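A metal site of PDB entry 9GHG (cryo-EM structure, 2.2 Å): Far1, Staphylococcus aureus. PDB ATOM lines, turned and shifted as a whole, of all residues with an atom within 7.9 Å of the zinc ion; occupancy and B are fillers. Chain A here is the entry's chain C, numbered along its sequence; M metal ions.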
ATOM      1  N   PHE A 119      34.519 -12.475  -9.044  1.00  0.00           N
ATOM      2  CA  PHE A 119      35.077 -11.380  -9.823  1.00  0.00           C
ATOM      3  C   PHE A 119      36.262 -10.795  -9.059  1.00  0.00           C
ATOM      4  O   PHE A 119      36.376 -11.021  -7.855  1.00  0.00           O
ATOM      5  CB  PHE A 119      33.994 -10.326 -10.069  1.00  0.00           C
ATOM      6  CG  PHE A 119      33.532  -9.590  -8.823  1.00  0.00           C
ATOM      7  CD1 PHE A 119      32.471 -10.066  -8.052  1.00  0.00           C
ATOM      8  CD2 PHE A 119      34.169  -8.419  -8.403  1.00  0.00           C
ATOM      9  CE1 PHE A 119      32.059  -9.394  -6.914  1.00  0.00           C
ATOM     10  CE2 PHE A 119      33.747  -7.753  -7.257  1.00  0.00           C
ATOM     11  CZ  PHE A 119      32.700  -8.241  -6.517  1.00  0.00           C
ATOM     12  N   GLY A 155      25.325   0.095   4.416  1.00  0.00           N
ATOM     13  CA  GLY A 155      24.165  -0.166   3.575  1.00  0.00           C
ATOM     14  C   GLY A 155      24.273  -1.515   2.879  1.00  0.00           C
ATOM     15  O   GLY A 155      25.355  -2.093   2.805  1.00  0.00           O
ATOM     16  N   PHE A 156      23.132  -1.999   2.360  1.00  0.00           N
ATOM     17  CA  PHE A 156      23.111  -3.235   1.590  1.00  0.00           C
ATOM     18  C   PHE A 156      23.798  -2.996   0.248  1.00  0.00           C
ATOM     19  O   PHE A 156      23.542  -1.982  -0.406  1.00  0.00           O
ATOM     20  CB  PHE A 156      21.655  -3.700   1.451  1.00  0.00           C
ATOM     21  CG  PHE A 156      21.056  -4.318   2.720  1.00  0.00           C
ATOM     22  CD1 PHE A 156      20.523  -3.507   3.717  1.00  0.00           C
ATOM     23  CD2 PHE A 156      21.009  -5.688   2.892  1.00  0.00           C
ATOM     24  CE1 PHE A 156      19.981  -4.062   4.859  1.00  0.00           C
ATOM     25  CE2 PHE A 156      20.467  -6.245   4.044  1.00  0.00           C
ATOM     26  CZ  PHE A 156      19.944  -5.426   5.023  1.00  0.00           C
ATOM     27  N   CYS A 157      24.669  -3.932  -0.158  1.00  0.00           N
ATOM     28  CA  CYS A 157      25.473  -3.786  -1.362  1.00  0.00           C
ATOM     29  C   CYS A 157      24.725  -4.375  -2.564  1.00  0.00           C
ATOM     30  O   CYS A 157      24.053  -5.396  -2.434  1.00  0.00           O
ATOM     31  CB  CYS A 157      26.834  -4.446  -1.180  1.00  0.00           C
ATOM     32  SG  CYS A 157      27.634  -4.940  -2.731  1.00  0.00           S
ATOM     33  N   THR A 158      24.881  -3.734  -3.738  1.00  0.00           N
ATOM     34  CA  THR A 158      24.154  -4.130  -4.937  1.00  0.00           C
ATOM     35  C   THR A 158      24.630  -5.499  -5.418  1.00  0.00           C
ATOM     36  O   THR A 158      23.812  -6.308  -5.848  1.00  0.00           O
ATOM     37  CB  THR A 158      24.324  -3.068  -6.021  1.00  0.00           C
ATOM     38  OG1 THR A 158      23.898  -1.844  -5.447  1.00  0.00           O
ATOM     39  CG2 THR A 158      23.510  -3.372  -7.264  1.00  0.00           C
ATOM     40  N   ILE A 159      25.945  -5.742  -5.376  1.00  0.00           N
ATOM     41  CA  ILE A 159      26.510  -6.959  -5.947  1.00  0.00           C
ATOM     42  C   ILE A 159      26.121  -8.155  -5.087  1.00  0.00           C
ATOM     43  O   ILE A 159      25.589  -9.138  -5.610  1.00  0.00           O
ATOM     44  CB  ILE A 159      28.032  -6.848  -6.155  1.00  0.00           C
ATOM     45  CG1 ILE A 159      28.393  -5.665  -7.070  1.00  0.00           C
ATOM     46  CG2 ILE A 159      28.602  -8.162  -6.680  1.00  0.00           C
ATOM     47  CD1 ILE A 159      29.877  -5.459  -7.276  1.00  0.00           C
ATOM     48  N   CYS A 160      26.372  -8.085  -3.771  1.00  0.00           N
ATOM     49  CA  CYS A 160      26.194  -9.239  -2.896  1.00  0.00           C
ATOM     50  C   CYS A 160      24.826  -9.248  -2.210  1.00  0.00           C
ATOM     51  O   CYS A 160      24.434 -10.271  -1.658  1.00  0.00           O
ATOM     52  CB  CYS A 160      27.314  -9.349  -1.864  1.00  0.00           C
ATOM     53  SG  CYS A 160      27.525  -7.870  -0.833  1.00  0.00           S
ATOM     54  N   ASN A 161      24.097  -8.113  -2.257  1.00  0.00           N
ATOM     55  CA  ASN A 161      22.793  -8.004  -1.608  1.00  0.00           C
ATOM     56  C   ASN A 161      22.919  -8.263  -0.112  1.00  0.00           C
ATOM     57  O   ASN A 161      22.021  -8.832   0.496  1.00  0.00           O
ATOM     58  CB  ASN A 161      21.758  -8.935  -2.250  1.00  0.00           C
ATOM     59  CG  ASN A 161      21.425  -8.544  -3.672  1.00  0.00           C
ATOM     60  OD1 ASN A 161      21.895  -7.512  -4.164  1.00  0.00           O
ATOM     61  ND2 ASN A 161      20.601  -9.345  -4.345  1.00  0.00           N
ATOM     62  N   LYS A 162      24.033  -7.816   0.480  1.00  0.00           N
ATOM     63  CA  LYS A 162      24.299  -7.988   1.901  1.00  0.00           C
ATOM     64  C   LYS A 162      24.623  -6.633   2.515  1.00  0.00           C
ATOM     65  O   LYS A 162      25.268  -5.806   1.864  1.00  0.00           O
ATOM     66  CB  LYS A 162      25.486  -8.925   2.155  1.00  0.00           C
ATOM     67  CG  LYS A 162      25.456 -10.281   1.456  1.00  0.00           C
ATOM     68  CD  LYS A 162      24.287 -11.187   1.842  1.00  0.00           C
ATOM     69  CE  LYS A 162      24.421 -12.555   1.268  1.00  0.00           C
ATOM     70  NZ  LYS A 162      24.541 -12.558  -0.196  1.00  0.00           N
ATOM     71  N   GLU A 163      24.206  -6.421   3.772  1.00  0.00           N
ATOM     72  CA  GLU A 163      24.541  -5.190   4.489  1.00  0.00           C
ATOM     73  C   GLU A 163      26.037  -5.195   4.790  1.00  0.00           C
ATOM     74  O   GLU A 163      26.538  -6.119   5.440  1.00  0.00           O
ATOM     75  CB  GLU A 163      23.701  -5.053   5.756  1.00  0.00           C
ATOM     76  CG  GLU A 163      23.561  -3.605   6.220  1.00  0.00           C
ATOM     77  CD  GLU A 163      22.590  -3.400   7.383  1.00  0.00           C
ATOM     78  OE1 GLU A 163      22.093  -4.407   7.928  1.00  0.00           O
ATOM     79  OE2 GLU A 163      22.331  -2.234   7.720  1.00  0.00           O
ATOM     80  N   SER A 164      26.738  -4.168   4.308  1.00  0.00           N
ATOM     81  CA  SER A 164      28.189  -4.099   4.412  1.00  0.00           C
ATOM     82  C   SER A 164      28.640  -2.642   4.353  1.00  0.00           C
ATOM     83  O   SER A 164      27.834  -1.753   4.096  1.00  0.00           O
ATOM     84  CB  SER A 164      28.849  -4.914   3.335  1.00  0.00           C
ATOM     85  OG  SER A 164      28.384  -6.254   3.331  1.00  0.00           O
ATOM     86  N   ASN A 165      29.935  -2.389   4.595  1.00  0.00           N
ATOM     87  CA  ASN A 165      30.509  -1.067   4.413  1.00  0.00           C
ATOM     88  C   ASN A 165      30.620  -0.819   2.907  1.00  0.00           C
ATOM     89  O   ASN A 165      31.373  -1.505   2.226  1.00  0.00           O
ATOM     90  CB  ASN A 165      31.863  -0.927   5.090  1.00  0.00           C
ATOM     91  CG  ASN A 165      31.842  -1.409   6.526  1.00  0.00           C
ATOM     92  OD1 ASN A 165      31.091  -0.880   7.345  1.00  0.00           O
ATOM     93  ND2 ASN A 165      32.659  -2.404   6.838  1.00  0.00           N
ATOM     94  N   VAL A 166      29.874   0.182   2.399  1.00  0.00           N
ATOM     95  CA  VAL A 166      29.728   0.362   0.960  1.00  0.00           C
ATOM     96  C   VAL A 166      30.070   1.804   0.583  1.00  0.00           C
ATOM     97  O   VAL A 166      30.043   2.699   1.427  1.00  0.00           O
ATOM     98  CB  VAL A 166      28.303  -0.014   0.493  1.00  0.00           C
ATOM     99  CG1 VAL A 166      28.045  -1.506   0.606  1.00  0.00           C
ATOM    100  CG2 VAL A 166      27.214   0.770   1.221  1.00  0.00           C
ATOM    101  N   TYR A 187      25.501   1.547  -4.742  1.00  0.00           N
ATOM    102  CA  TYR A 187      26.298   1.327  -3.545  1.00  0.00           C
ATOM    103  C   TYR A 187      26.819  -0.108  -3.544  1.00  0.00           C
ATOM    104  O   TYR A 187      26.026  -1.053  -3.536  1.00  0.00           O
ATOM    105  CB  TYR A 187      25.488   1.641  -2.277  1.00  0.00           C
ATOM    106  CG  TYR A 187      25.401   3.124  -1.945  1.00  0.00           C
ATOM    107  CD1 TYR A 187      24.353   3.911  -2.424  1.00  0.00           C
ATOM    108  CD2 TYR A 187      26.357   3.734  -1.138  1.00  0.00           C
ATOM    109  CE1 TYR A 187      24.273   5.258  -2.113  1.00  0.00           C
ATOM    110  CE2 TYR A 187      26.277   5.080  -0.827  1.00  0.00           C
ATOM    111  CZ  TYR A 187      25.245   5.843  -1.308  1.00  0.00           C
ATOM    112  OH  TYR A 187      25.168   7.167  -1.000  1.00  0.00           O
ATOM    113  N   ILE A 188      28.148  -0.264  -3.558  1.00  0.00           N
ATOM    114  CA  ILE A 188      28.784  -1.574  -3.568  1.00  0.00           C
ATOM    115  C   ILE A 188      29.862  -1.597  -2.485  1.00  0.00           C
ATOM    116  O   ILE A 188      30.334  -0.547  -2.059  1.00  0.00           O
ATOM    117  CB  ILE A 188      29.351  -1.903  -4.962  1.00  0.00           C
ATOM    118  CG1 ILE A 188      30.522  -0.985  -5.336  1.00  0.00           C
ATOM    119  CG2 ILE A 188      28.243  -1.879  -6.017  1.00  0.00           C
ATOM    120  CD1 ILE A 188      31.200  -1.345  -6.644  1.00  0.00           C
ATOM    121  N   CYS A 189      30.248  -2.805  -2.044  1.00  0.00           N
ATOM    122  CA  CYS A 189      31.253  -2.979  -1.013  1.00  0.00           C
ATOM    123  C   CYS A 189      32.571  -2.330  -1.448  1.00  0.00           C
ATOM    124  O   CYS A 189      32.984  -2.497  -2.586  1.00  0.00           O
ATOM    125  CB  CYS A 189      31.524  -4.452  -0.716  1.00  0.00           C
ATOM    126  SG  CYS A 189      30.076  -5.357  -0.132  1.00  0.00           S
ATOM    127  N   ARG A 190      33.212  -1.604  -0.519  1.00  0.00           N
ATOM    128  CA  ARG A 190      34.489  -0.973  -0.808  1.00  0.00           C
ATOM    129  C   ARG A 190      35.556  -2.053  -1.005  1.00  0.00           C
ATOM    130  O   ARG A 190      36.400  -1.938  -1.885  1.00  0.00           O
ATOM    131  CB  ARG A 190      34.908   0.037   0.268  1.00  0.00           C
ATOM    132  CG  ARG A 190      35.888   1.072  -0.257  1.00  0.00           C
ATOM    133  CD  ARG A 190      36.459   2.005   0.790  1.00  0.00           C
ATOM    134  NE  ARG A 190      37.203   3.090   0.138  1.00  0.00           N
ATOM    135  CZ  ARG A 190      36.654   4.073  -0.578  1.00  0.00           C
ATOM    136  NH1 ARG A 190      35.370   4.368  -0.456  1.00  0.00           N
ATOM    137  NH2 ARG A 190      37.422   4.791  -1.378  1.00  0.00           N
ATOM    138  N   ASP A 191      35.498  -3.101  -0.172  1.00  0.00           N
ATOM    139  CA  ASP A 191      36.371  -4.253  -0.317  1.00  0.00           C
ATOM    140  C   ASP A 191      35.690  -5.286  -1.208  1.00  0.00           C
ATOM    141  O   ASP A 191      34.663  -5.844  -0.833  1.00  0.00           O
ATOM    142  CB  ASP A 191      36.738  -4.844   1.035  1.00  0.00           C
ATOM    143  CG  ASP A 191      37.779  -5.959   1.023  1.00  0.00           C
ATOM    144  OD1 ASP A 191      38.330  -6.245  -0.060  1.00  0.00           O
ATOM    145  OD2 ASP A 191      38.041  -6.531   2.105  1.00  0.00           O
ATOM    146  N   SER A 192      36.265  -5.521  -2.393  1.00  0.00           N
ATOM    147  CA  SER A 192      35.724  -6.467  -3.358  1.00  0.00           C
ATOM    148  C   SER A 192      35.926  -7.908  -2.879  1.00  0.00           C
ATOM    149  O   SER A 192      35.097  -8.763  -3.165  1.00  0.00           O
ATOM    150  CB  SER A 192      36.332  -6.266  -4.724  1.00  0.00           C
ATOM    151  OG  SER A 192      36.147  -4.937  -5.178  1.00  0.00           O
ATOM    152  N   HIS A 194      35.975  -9.019   0.262  1.00  0.00           N
ATOM    153  CA  HIS A 194      34.931  -9.264   1.235  1.00  0.00           C
ATOM    154  C   HIS A 194      33.593  -9.474   0.518  1.00  0.00           C
ATOM    155  O   HIS A 194      32.809 -10.342   0.906  1.00  0.00           O
ATOM    156  CB  HIS A 194      34.849  -8.135   2.263  1.00  0.00           C
ATOM    157  CG  HIS A 194      33.822  -8.342   3.335  1.00  0.00           C
ATOM    158  ND1 HIS A 194      33.481  -9.588   3.805  1.00  0.00           N
ATOM    159  CD2 HIS A 194      33.082  -7.468   4.017  1.00  0.00           C
ATOM    160  CE1 HIS A 194      32.547  -9.468   4.744  1.00  0.00           C
ATOM    161  NE2 HIS A 194      32.288  -8.186   4.886  1.00  0.00           N
ATOM    162  N   CYS A 195      33.356  -8.672  -0.524  1.00  0.00           N
ATOM    163  CA  CYS A 195      32.160  -8.790  -1.346  1.00  0.00           C
ATOM    164  C   CYS A 195      32.061 -10.176  -1.964  1.00  0.00           C
ATOM    165  O   CYS A 195      30.977 -10.767  -1.997  1.00  0.00           O
ATOM    166  CB  CYS A 195      32.149  -7.736  -2.459  1.00  0.00           C
ATOM    167  SG  CYS A 195      30.582  -7.647  -3.352  1.00  0.00           S
ATOM    168  N   ASN A 196      33.193 -10.702  -2.463  1.00  0.00           N
ATOM    169  CA  ASN A 196      33.229 -12.007  -3.117  1.00  0.00           C
ATOM    170  C   ASN A 196      32.839 -13.108  -2.131  1.00  0.00           C
ATOM    171  O   ASN A 196      32.136 -14.038  -2.508  1.00  0.00           O
ATOM    172  CB  ASN A 196      34.596 -12.283  -3.727  1.00  0.00           C
ATOM    173  CG  ASN A 196      34.846 -11.464  -4.976  1.00  0.00           C
ATOM    174  OD1 ASN A 196      34.118 -11.605  -5.961  1.00  0.00           O
ATOM    175  ND2 ASN A 196      35.857 -10.606  -4.958  1.00  0.00           N
ATOM    176  N   LYS A 197      33.309 -12.982  -0.887  1.00  0.00           N
ATOM    177  CA  LYS A 197      33.014 -13.965   0.148  1.00  0.00           C
ATOM    178  C   LYS A 197      31.514 -13.951   0.449  1.00  0.00           C
ATOM    179  O   LYS A 197      30.897 -15.010   0.608  1.00  0.00           O
ATOM    180  CB  LYS A 197      33.787 -13.669   1.437  1.00  0.00           C
ATOM    181  CG  LYS A 197      35.303 -13.569   1.298  1.00  0.00           C
ATOM    182  CD  LYS A 197      35.975 -12.896   2.486  1.00  0.00           C
ATOM    183  CE  LYS A 197      37.426 -12.623   2.237  1.00  0.00           C
ATOM    184  NZ  LYS A 197      38.027 -11.842   3.313  1.00  0.00           N
ATOM    185  N   GLN A 198      30.944 -12.749   0.539  1.00  0.00           N
ATOM    186  CA  GLN A 198      29.535 -12.571   0.885  1.00  0.00           C
ATOM    187  C   GLN A 198      28.633 -13.052  -0.253  1.00  0.00           C
ATOM    188  O   GLN A 198      27.553 -13.584  -0.001  1.00  0.00           O
ATOM    189  CB  GLN A 198      29.241 -11.103   1.216  1.00  0.00           C
ATOM    190  CG  GLN A 198      29.961 -10.597   2.462  1.00  0.00           C
ATOM    191  CD  GLN A 198      29.776  -9.119   2.693  1.00  0.00           C
ATOM    192  OE1 GLN A 198      29.239  -8.686   3.720  1.00  0.00           O
ATOM    193  NE2 GLN A 198      30.225  -8.308   1.746  1.00  0.00           N
ATOM    194  N   LEU A 199      29.070 -12.842  -1.511  1.00  0.00           N
ATOM    195  CA  LEU A 199      28.267 -13.207  -2.671  1.00  0.00           C
ATOM    196  C   LEU A 199      28.077 -14.723  -2.709  1.00  0.00           C
ATOM    197  O   LEU A 199      29.037 -15.473  -2.578  1.00  0.00           O
ATOM    198  CB  LEU A 199      28.956 -12.710  -3.941  1.00  0.00           C
ATOM    199  CG  LEU A 199      28.172 -12.893  -5.243  1.00  0.00           C
ATOM    200  CD1 LEU A 199      26.905 -12.047  -5.224  1.00  0.00           C
ATOM    201  CD2 LEU A 199      29.020 -12.548  -6.462  1.00  0.00           C
HETATM  202 ZN    ZN M   1      29.149  -6.585  -1.900  1.00  0.00          ZN
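The zinc ion is bound by the side-chain sulfur (SG) of Cys 195 (2.3 Å), the side-chain sulfur (SG) of Cys 160 (2.3 Å), the side-chain sulfur (SG) of Cys 189 (2.3 Å) and the side-chain sulfur (SG) of Cys 157 (2.4 Å).
The side-chain sulfur of Cys 160 sits close to the side-chain amide nitrogen of Gln 198 (3.8 Å).
O of Cys 160 sits at hydrogen-bond distance from NZ of Lys 162.
SG of Cys 189 sits close to NE2 of Gln 198, at 3.5 Å.
The backbone NH of Ile 159 lies close to the side-chain sulfur of Cys 157.
O of Cys 157 lies close to OD1 of Asn 161.
The backbone NH (N) of Cys 157 is in hydrogen-bond range of the backbone carbonyl oxygen (O) of Lys 162 (2.8 Å).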
